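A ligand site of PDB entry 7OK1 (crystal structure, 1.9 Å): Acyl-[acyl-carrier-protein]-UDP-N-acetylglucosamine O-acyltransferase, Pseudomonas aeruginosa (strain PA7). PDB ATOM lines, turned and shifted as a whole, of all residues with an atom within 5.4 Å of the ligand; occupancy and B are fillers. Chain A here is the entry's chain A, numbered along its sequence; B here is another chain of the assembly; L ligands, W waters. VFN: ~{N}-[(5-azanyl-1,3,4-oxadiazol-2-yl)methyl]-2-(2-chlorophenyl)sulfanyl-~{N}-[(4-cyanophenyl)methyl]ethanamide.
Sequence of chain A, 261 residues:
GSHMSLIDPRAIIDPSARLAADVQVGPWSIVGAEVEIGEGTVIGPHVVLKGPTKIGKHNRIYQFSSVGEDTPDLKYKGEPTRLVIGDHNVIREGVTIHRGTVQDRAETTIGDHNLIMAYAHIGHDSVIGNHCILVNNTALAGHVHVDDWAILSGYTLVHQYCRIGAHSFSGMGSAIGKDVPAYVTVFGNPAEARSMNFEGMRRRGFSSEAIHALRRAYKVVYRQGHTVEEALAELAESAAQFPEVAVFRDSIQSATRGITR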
ATOM      1  N   PRO A  72     -19.248   3.498 -26.799  1.00  0.00           N
ATOM      2  CA  PRO A  72     -18.541   3.614 -28.083  1.00  0.00           C
ATOM      3  C   PRO A  72     -17.414   4.644 -28.047  1.00  0.00           C
ATOM      4  O   PRO A  72     -16.595   4.646 -28.961  1.00  0.00           O
ATOM      5  CB  PRO A  72     -19.652   4.063 -29.048  1.00  0.00           C
ATOM      6  CG  PRO A  72     -20.594   4.841 -28.201  1.00  0.00           C
ATOM      7  CD  PRO A  72     -20.559   4.193 -26.833  1.00  0.00           C
ATOM      8  N   ASP A  73     -17.393   5.542 -27.026  1.00  0.00           N
ATOM      9  CA  ASP A  73     -16.408   6.619 -26.847  1.00  0.00           C
ATOM     10  C   ASP A  73     -14.968   6.145 -27.084  1.00  0.00           C
ATOM     11  O   ASP A  73     -14.513   5.197 -26.442  1.00  0.00           O
ATOM     12  CB  ASP A  73     -16.564   7.325 -25.474  1.00  0.00           C
ATOM     13  CG  ASP A  73     -17.828   8.160 -25.293  1.00  0.00           C
ATOM     14  OD1 ASP A  73     -18.654   8.216 -26.236  1.00  0.00           O
ATOM     15  OD2 ASP A  73     -17.985   8.748 -24.216  1.00  0.00           O
ATOM     16  N   LEU A  74     -14.295   6.766 -28.070  1.00  0.00           N
ATOM     17  CA  LEU A  74     -12.952   6.430 -28.578  1.00  0.00           C
ATOM     18  C   LEU A  74     -11.867   6.217 -27.489  1.00  0.00           C
ATOM     19  O   LEU A  74     -10.881   5.514 -27.745  1.00  0.00           O
ATOM     20  CB  LEU A  74     -12.493   7.493 -29.596  1.00  0.00           C
ATOM     21  CG  LEU A  74     -13.022   7.419 -31.059  1.00  0.00           C
ATOM     22  CD1 LEU A  74     -13.865   6.177 -31.364  1.00  0.00           C
ATOM     23  CD2 LEU A  74     -13.744   8.656 -31.414  1.00  0.00           C
ATOM     24  N   HIS A 121     -30.858   7.234 -22.084  1.00  0.00           N
ATOM     25  CA  HIS A 121     -29.468   6.836 -22.226  1.00  0.00           C
ATOM     26  C   HIS A 121     -28.688   7.174 -20.998  1.00  0.00           C
ATOM     27  O   HIS A 121     -28.681   8.334 -20.563  1.00  0.00           O
ATOM     28  CB  HIS A 121     -28.814   7.486 -23.447  1.00  0.00           C
ATOM     29  CG  HIS A 121     -27.335   7.282 -23.508  1.00  0.00           C
ATOM     30  ND1 HIS A 121     -26.793   6.083 -23.970  1.00  0.00           N
ATOM     31  CD2 HIS A 121     -26.334   8.094 -23.104  1.00  0.00           C
ATOM     32  CE1 HIS A 121     -25.477   6.233 -23.885  1.00  0.00           C
ATOM     33  NE2 HIS A 121     -25.155   7.418 -23.352  1.00  0.00           N
ATOM     34  N   HIS A 124     -21.407   6.047 -19.763  1.00  0.00           N
ATOM     35  CA  HIS A 124     -20.343   5.507 -18.901  1.00  0.00           C
ATOM     36  C   HIS A 124     -20.087   6.333 -17.631  1.00  0.00           C
ATOM     37  O   HIS A 124     -20.087   7.576 -17.674  1.00  0.00           O
ATOM     38  CB  HIS A 124     -19.025   5.292 -19.685  1.00  0.00           C
ATOM     39  CG  HIS A 124     -18.441   6.542 -20.265  1.00  0.00           C
ATOM     40  ND1 HIS A 124     -17.425   7.231 -19.624  1.00  0.00           N
ATOM     41  CD2 HIS A 124     -18.738   7.192 -21.413  1.00  0.00           C
ATOM     42  CE1 HIS A 124     -17.124   8.248 -20.402  1.00  0.00           C
ATOM     43  NE2 HIS A 124     -17.887   8.282 -21.481  1.00  0.00           N
ATOM     44  N   ALA A 139     -30.861  11.845 -21.785  1.00  0.00           N
ATOM     45  CA  ALA A 139     -29.541  11.320 -22.090  1.00  0.00           C
ATOM     46  C   ALA A 139     -28.509  11.922 -21.187  1.00  0.00           C
ATOM     47  O   ALA A 139     -28.432  13.156 -21.060  1.00  0.00           O
ATOM     48  CB  ALA A 139     -29.196  11.592 -23.562  1.00  0.00           C
ATOM     49  N   LEU A 140     -27.750  11.048 -20.487  1.00  0.00           N
ATOM     50  CA  LEU A 140     -26.657  11.414 -19.588  1.00  0.00           C
ATOM     51  C   LEU A 140     -25.415  11.086 -20.389  1.00  0.00           C
ATOM     52  O   LEU A 140     -25.155   9.928 -20.654  1.00  0.00           O
ATOM     53  CB  LEU A 140     -26.672  10.623 -18.241  1.00  0.00           C
ATOM     54  CG  LEU A 140     -27.995  10.506 -17.442  1.00  0.00           C
ATOM     55  CD1 LEU A 140     -27.736   9.883 -16.047  1.00  0.00           C
ATOM     56  CD2 LEU A 140     -28.704  11.878 -17.261  1.00  0.00           C
ATOM     57  N   ALA A 141     -24.678  12.116 -20.818  1.00  0.00           N
ATOM     58  CA  ALA A 141     -23.487  11.950 -21.679  1.00  0.00           C
ATOM     59  C   ALA A 141     -22.403  11.047 -21.098  1.00  0.00           C
ATOM     60  O   ALA A 141     -21.766  10.315 -21.840  1.00  0.00           O
ATOM     61  CB  ALA A 141     -22.906  13.302 -22.059  1.00  0.00           C
ATOM     62  N   GLY A 142     -22.224  11.073 -19.791  1.00  0.00           N
ATOM     63  CA  GLY A 142     -21.187  10.313 -19.110  1.00  0.00           C
ATOM     64  C   GLY A 142     -20.716  11.033 -17.868  1.00  0.00           C
ATOM     65  O   GLY A 142     -20.724  12.271 -17.816  1.00  0.00           O
ATOM     66  N   LEU A 157     -31.171  16.582 -21.681  1.00  0.00           N
ATOM     67  CA  LEU A 157     -29.820  16.229 -22.109  1.00  0.00           C
ATOM     68  C   LEU A 157     -28.886  16.760 -21.088  1.00  0.00           C
ATOM     69  O   LEU A 157     -29.007  17.925 -20.697  1.00  0.00           O
ATOM     70  CB  LEU A 157     -29.527  16.824 -23.490  1.00  0.00           C
ATOM     71  CG  LEU A 157     -30.558  16.550 -24.597  1.00  0.00           C
ATOM     72  CD1 LEU A 157     -30.117  17.192 -25.899  1.00  0.00           C
ATOM     73  CD2 LEU A 157     -30.799  15.031 -24.771  1.00  0.00           C
ATOM     74  N   VAL A 158     -27.994  15.878 -20.582  1.00  0.00           N
ATOM     75  CA  VAL A 158     -27.076  16.274 -19.521  1.00  0.00           C
ATOM     76  C   VAL A 158     -25.645  16.106 -19.963  1.00  0.00           C
ATOM     77  O   VAL A 158     -25.226  15.001 -20.324  1.00  0.00           O
ATOM     78  CB  VAL A 158     -27.378  15.571 -18.166  1.00  0.00           C
ATOM     79  CG1 VAL A 158     -26.521  16.167 -17.035  1.00  0.00           C
ATOM     80  CG2 VAL A 158     -28.873  15.696 -17.808  1.00  0.00           C
ATOM     81  N   GLN A 160     -21.503  15.959 -19.798  1.00  0.00           N
ATOM     82  CA  GLN A 160     -20.577  15.157 -19.001  1.00  0.00           C
ATOM     83  C   GLN A 160     -20.164  15.891 -17.736  1.00  0.00           C
ATOM     84  O   GLN A 160     -19.985  17.120 -17.733  1.00  0.00           O
ATOM     85  CB  GLN A 160     -19.303  14.840 -19.785  1.00  0.00           C
ATOM     86  CG  GLN A 160     -19.497  13.793 -20.861  1.00  0.00           C
ATOM     87  CD  GLN A 160     -18.181  13.141 -21.121  1.00  0.00           C
ATOM     88  OE1 GLN A 160     -17.934  12.000 -20.709  1.00  0.00           O
ATOM     89  NE2 GLN A 160     -17.286  13.866 -21.795  1.00  0.00           N
ATOM     90  N   LEU B 115     -18.362   6.866 -36.731  1.00  0.00           N
ATOM     91  CA  LEU B 115     -18.970   6.406 -35.476  1.00  0.00           C
ATOM     92  C   LEU B 115     -20.363   7.047 -35.414  1.00  0.00           C
ATOM     93  O   LEU B 115     -20.510   8.264 -35.283  1.00  0.00           O
ATOM     94  CB  LEU B 115     -18.092   6.774 -34.266  1.00  0.00           C
ATOM     95  CG  LEU B 115     -18.624   6.461 -32.856  1.00  0.00           C
ATOM     96  CD1 LEU B 115     -19.030   4.973 -32.715  1.00  0.00           C
ATOM     97  CD2 LEU B 115     -17.598   6.832 -31.826  1.00  0.00           C
ATOM     98  N   MET B 117     -23.692   6.801 -33.456  1.00  0.00           N
ATOM     99  CA  MET B 117     -24.139   6.350 -32.152  1.00  0.00           C
ATOM    100  C   MET B 117     -25.634   6.095 -32.063  1.00  0.00           C
ATOM    101  O   MET B 117     -26.342   6.366 -33.010  1.00  0.00           O
ATOM    102  CB  MET B 117     -23.634   7.273 -31.054  1.00  0.00           C
ATOM    103  CG  MET B 117     -22.116   7.157 -30.850  1.00  0.00           C
ATOM    104  SD  MET B 117     -21.327   8.426 -29.807  1.00  0.00           S
ATOM    105  CE  MET B 117     -22.136   8.237 -28.414  1.00  0.00           C
ATOM    106  N   ILE B 133     -18.302  11.731 -36.376  1.00  0.00           N
ATOM    107  CA  ILE B 133     -18.974  11.265 -35.180  1.00  0.00           C
ATOM    108  C   ILE B 133     -20.339  11.892 -35.139  1.00  0.00           C
ATOM    109  O   ILE B 133     -20.471  13.126 -35.143  1.00  0.00           O
ATOM    110  CB  ILE B 133     -18.190  11.451 -33.861  1.00  0.00           C
ATOM    111  CG1 ILE B 133     -16.764  10.827 -33.942  1.00  0.00           C
ATOM    112  CG2 ILE B 133     -18.983  10.871 -32.661  1.00  0.00           C
ATOM    113  CD1 ILE B 133     -15.788  11.258 -32.792  1.00  0.00           C
ATOM    114  N   VAL B 135     -23.314  11.612 -32.682  1.00  0.00           N
ATOM    115  CA  VAL B 135     -23.596  11.173 -31.321  1.00  0.00           C
ATOM    116  C   VAL B 135     -25.082  10.816 -31.199  1.00  0.00           C
ATOM    117  O   VAL B 135     -25.835  11.149 -32.108  1.00  0.00           O
ATOM    118  CB  VAL B 135     -23.085  12.258 -30.332  1.00  0.00           C
ATOM    119  CG1 VAL B 135     -23.308  11.880 -28.867  1.00  0.00           C
ATOM    120  CG2 VAL B 135     -21.601  12.525 -30.577  1.00  0.00           C
ATOM    121  N   ASN B 136     -25.485  10.094 -30.131  1.00  0.00           N
ATOM    122  CA  ASN B 136     -26.853   9.637 -29.904  1.00  0.00           C
ATOM    123  C   ASN B 136     -27.952  10.544 -30.412  1.00  0.00           C
ATOM    124  O   ASN B 136     -27.966  11.742 -30.089  1.00  0.00           O
ATOM    125  CB  ASN B 136     -27.130   9.409 -28.428  1.00  0.00           C
ATOM    126  CG  ASN B 136     -26.294   8.358 -27.788  1.00  0.00           C
ATOM    127  OD1 ASN B 136     -25.125   8.241 -28.078  1.00  0.00           O
ATOM    128  ND2 ASN B 136     -26.890   7.601 -26.872  1.00  0.00           N
ATOM    129  N   ILE B 151     -18.093  16.536 -36.018  1.00  0.00           N
ATOM    130  CA  ILE B 151     -18.672  15.949 -34.802  1.00  0.00           C
ATOM    131  C   ILE B 151     -20.013  16.612 -34.589  1.00  0.00           C
ATOM    132  O   ILE B 151     -20.076  17.839 -34.499  1.00  0.00           O
ATOM    133  CB  ILE B 151     -17.797  16.082 -33.511  1.00  0.00           C
ATOM    134  CG1 ILE B 151     -16.497  15.252 -33.609  1.00  0.00           C
ATOM    135  CG2 ILE B 151     -18.609  15.701 -32.250  1.00  0.00           C
ATOM    136  CD1 ILE B 151     -15.370  15.697 -32.598  1.00  0.00           C
ATOM    137  N   LEU B 152     -21.095  15.815 -34.533  1.00  0.00           N
ATOM    138  CA  LEU B 152     -22.439  16.334 -34.227  1.00  0.00           C
ATOM    139  C   LEU B 152     -22.821  15.748 -32.876  1.00  0.00           C
ATOM    140  O   LEU B 152     -22.976  14.545 -32.738  1.00  0.00           O
ATOM    141  CB  LEU B 152     -23.469  15.982 -35.327  1.00  0.00           C
ATOM    142  CG  LEU B 152     -23.207  16.530 -36.750  1.00  0.00           C
ATOM    143  CD1 LEU B 152     -24.120  15.869 -37.738  1.00  0.00           C
ATOM    144  CD2 LEU B 152     -23.434  18.061 -36.827  1.00  0.00           C
ATOM    145  N   SER B 153     -22.894  16.606 -31.847  1.00  0.00           N
ATOM    146  CA  SER B 153     -23.200  16.173 -30.489  1.00  0.00           C
ATOM    147  C   SER B 153     -24.592  15.606 -30.358  1.00  0.00           C
ATOM    148  O   SER B 153     -25.399  15.764 -31.267  1.00  0.00           O
ATOM    149  CB  SER B 153     -22.988  17.311 -29.489  1.00  0.00           C
ATOM    150  OG  SER B 153     -21.632  17.672 -29.372  1.00  0.00           O
ATOM    151  N   GLY B 154     -24.841  14.927 -29.247  1.00  0.00           N
ATOM    152  CA  GLY B 154     -26.102  14.265 -28.962  1.00  0.00           C
ATOM    153  C   GLY B 154     -27.318  15.103 -29.288  1.00  0.00           C
ATOM    154  O   GLY B 154     -27.397  16.260 -28.869  1.00  0.00           O
ATOM    155  N   TYR B 155     -28.245  14.524 -30.097  1.00  0.00           N
ATOM    156  CA  TYR B 155     -29.529  15.142 -30.462  1.00  0.00           C
ATOM    157  C   TYR B 155     -29.399  16.372 -31.360  1.00  0.00           C
ATOM    158  O   TYR B 155     -30.227  17.282 -31.284  1.00  0.00           O
ATOM    159  CB  TYR B 155     -30.343  15.459 -29.178  1.00  0.00           C
ATOM    160  CG  TYR B 155     -30.831  14.240 -28.435  1.00  0.00           C
ATOM    161  CD1 TYR B 155     -29.939  13.388 -27.756  1.00  0.00           C
ATOM    162  CD2 TYR B 155     -32.182  13.916 -28.405  1.00  0.00           C
ATOM    163  CE1 TYR B 155     -30.385  12.252 -27.086  1.00  0.00           C
ATOM    164  CE2 TYR B 155     -32.647  12.790 -27.729  1.00  0.00           C
ATOM    165  CZ  TYR B 155     -31.757  11.975 -27.047  1.00  0.00           C
ATOM    166  OH  TYR B 155     -32.275  10.898 -26.381  1.00  0.00           O
ATOM    167  N   PHE B 169     -18.262  21.397 -35.581  1.00  0.00           N
ATOM    168  CA  PHE B 169     -18.770  20.838 -34.336  1.00  0.00           C
ATOM    169  C   PHE B 169     -20.123  21.409 -33.994  1.00  0.00           C
ATOM    170  O   PHE B 169     -20.356  22.604 -34.133  1.00  0.00           O
ATOM    171  CB  PHE B 169     -17.765  21.085 -33.189  1.00  0.00           C
ATOM    172  CG  PHE B 169     -18.196  20.588 -31.836  1.00  0.00           C
ATOM    173  CD1 PHE B 169     -17.957  19.274 -31.446  1.00  0.00           C
ATOM    174  CD2 PHE B 169     -18.845  21.433 -30.936  1.00  0.00           C
ATOM    175  CE1 PHE B 169     -18.349  18.821 -30.178  1.00  0.00           C
ATOM    176  CE2 PHE B 169     -19.237  20.979 -29.668  1.00  0.00           C
ATOM    177  CZ  PHE B 169     -18.975  19.673 -29.301  1.00  0.00           C
ATOM    178  N   MET B 172     -24.692  19.836 -27.987  1.00  0.00           N
ATOM    179  CA  MET B 172     -25.868  18.971 -27.804  1.00  0.00           C
ATOM    180  C   MET B 172     -27.190  19.750 -27.943  1.00  0.00           C
ATOM    181  O   MET B 172     -27.287  20.908 -27.550  1.00  0.00           O
ATOM    182  CB  MET B 172     -25.808  18.145 -26.506  1.00  0.00           C
ATOM    183  CG  MET B 172     -25.877  18.951 -25.252  1.00  0.00           C
ATOM    184  SD  MET B 172     -25.989  17.940 -23.740  1.00  0.00           S
ATOM    185  CE  MET B 172     -26.612  19.126 -22.698  1.00  0.00           C
HETATM  186  C15 VFN L   1     -16.808  10.121 -28.811  1.00  0.00           C
HETATM  187  C23 VFN L   1     -23.197  10.966 -25.421  1.00  0.00           C
HETATM  188  C24 VFN L   1     -24.500  10.437 -25.419  1.00  0.00           C
HETATM  189  C11 VFN L   1     -16.944  12.532 -29.154  1.00  0.00           C
HETATM  190  C13 VFN L   1     -18.727  11.359 -27.979  1.00  0.00           C
HETATM  191  C10 VFN L   1     -17.620  13.751 -28.996  1.00  0.00           C
HETATM  192  C14 VFN L   1     -19.408  12.577 -27.830  1.00  0.00           C
HETATM  193  C22 VFN L   1     -22.990  12.351 -25.435  1.00  0.00           C
HETATM  194  C25 VFN L   1     -25.612  11.291 -25.413  1.00  0.00           C
HETATM  195  C12 VFN L   1     -17.500  11.352 -28.637  1.00  0.00           C
HETATM  196  C9  VFN L   1     -18.857  13.776 -28.327  1.00  0.00           C
HETATM  197  C21 VFN L   1     -24.105  13.217 -25.442  1.00  0.00           C
HETATM  198  C26 VFN L   1     -25.405  12.676 -25.428  1.00  0.00           C
HETATM  199  C5  VFN L   1     -18.773  14.193 -25.158  1.00  0.00           C
HETATM  200  C2  VFN L   1     -18.813  12.228 -24.359  1.00  0.00           C
HETATM  201  C17 VFN L   1     -21.548  15.087 -26.768  1.00  0.00           C
HETATM  202  C8  VFN L   1     -19.541  15.103 -28.147  1.00  0.00           C
HETATM  203  C6  VFN L   1     -19.350  15.472 -25.623  1.00  0.00           C
HETATM  204  C19 VFN L   1     -22.172  15.252 -25.410  1.00  0.00           C
HETATM  205  N16 VFN L   1     -16.261   9.108 -28.971  1.00  0.00           N
HETATM  206  N4  VFN L   1     -17.540  13.759 -25.220  1.00  0.00           N
HETATM  207  N3  VFN L   1     -17.553  12.478 -24.689  1.00  0.00           N
HETATM  208  N1  VFN L   1     -19.394  11.115 -23.812  1.00  0.00           N
HETATM  209  N7  VFN L   1     -20.169  15.243 -26.826  1.00  0.00           N
HETATM  210  O18 VFN L   1     -22.248  14.807 -27.732  1.00  0.00           O
HETATM  211  O28 VFN L   1     -19.642  13.287 -24.621  1.00  0.00           O
HETATM  212  S20 VFN L   1     -23.970  14.990 -25.484  1.00  0.00           S
HETATM  213 CL1  VFN L   1     -26.755  13.749 -25.411  1.00  0.00          CL
HETATM  214  O   HOH W   1     -22.597   8.259 -23.495  1.00  0.00           O
HETATM  215  O   HOH W   2     -21.352  18.487 -26.806  1.00  0.00           O
HETATM  216  O   HOH W   3     -17.800  16.900 -22.905  1.00  0.00           O
HETATM  217  O   HOH W   4     -20.585  16.677 -22.641  1.00  0.00           O
HETATM  218  O   HOH W   5     -18.716  18.757 -25.505  1.00  0.00           O
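The backbone NH (N) of Gly 154 of chain B sits at hydrogen-bond distance from an oxygen (O18) of the ligand, at 3.0 Å.
The backbone carbonyl oxygen (O) of Ala 141 is in hydrogen-bond range of a nitrogen (N1) of the ligand (3.2 Å).
OG of Ser 153 of chain B lies close to O18 of the ligand (3.4 Å).
N of Leu 74 sits at hydrogen-bond distance from N16 of the ligand, 3.2 Å away.
The side-chain amide nitrogen of Gln 160 sits at hydrogen-bond distance from a nitrogen (N3) of the ligand, at 3.2 Å.
The side-chain carboxylate (OD2) of Asp 73 is in hydrogen-bond range of a nitrogen (N1) of the ligand, 2.8 Å away.
The backbone carbonyl oxygen (O) of Ala 139 sits at hydrogen-bond distance from the backbone NH (N) of Val 158.
The backbone NH (N) of Ala 141 is in hydrogen-bond range of the backbone carbonyl oxygen (O) of Val 158 (3.0 Å).
N of Leu 140 is in hydrogen-bond range of O of His 121.
The backbone NH of Tyr 155 of chain B is in hydrogen-bond range of the backbone carbonyl oxygen of Asn 136 of chain B (2.8 Å).
The side-chain carboxylate of Asp 73 sits at hydrogen-bond distance from a ring nitrogen (NE2) of His 124 (2.8 Å).
The side-chain amide nitrogen (ND2) of Asn 136 of chain B lies within hydrogen-bond range of a ring nitrogen (ND1) of His 121 (3.3 Å).
His 121 touches the ligand (NE2 to C24, 3.7 Å).
His 124 touches the ligand (NE2 to N1, 3.97 Å).
Ala 139 touches the ligand (CB to CL1, 3.7 Å).
CD2 of Leu 115 of chain B touches N16 of the ligand, 3.9 Å away.
Val 135 of chain B touches the ligand.
OD1 of Asn 136 of chain B touches C24 of the ligand, 3.5 Å away.
Ile 151 of chain B touches the ligand (CG2 to C10, 3.9 Å).
CD1 of Tyr 155 of chain B touches CL1 of the ligand (3.97 Å).
Met 172 of chain B touches the ligand.
15 residues have an atom within 4 Å of the ligand: Asp 73, Leu 74, His 121, His 124, Ala 139, Ala 141, Gln 160, Leu 115 of chain B, Val 135 of chain B, Asn 136 of chain B, Ile 151 of chain B, Ser 153 of chain B, Gly 154 of chain B, Tyr 155 of chain B and Met 172 of chain B.
Water W1 bridges a ring nitrogen (NE2) of His 121 and the backbone carbonyl oxygen (O) of Ala 141.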
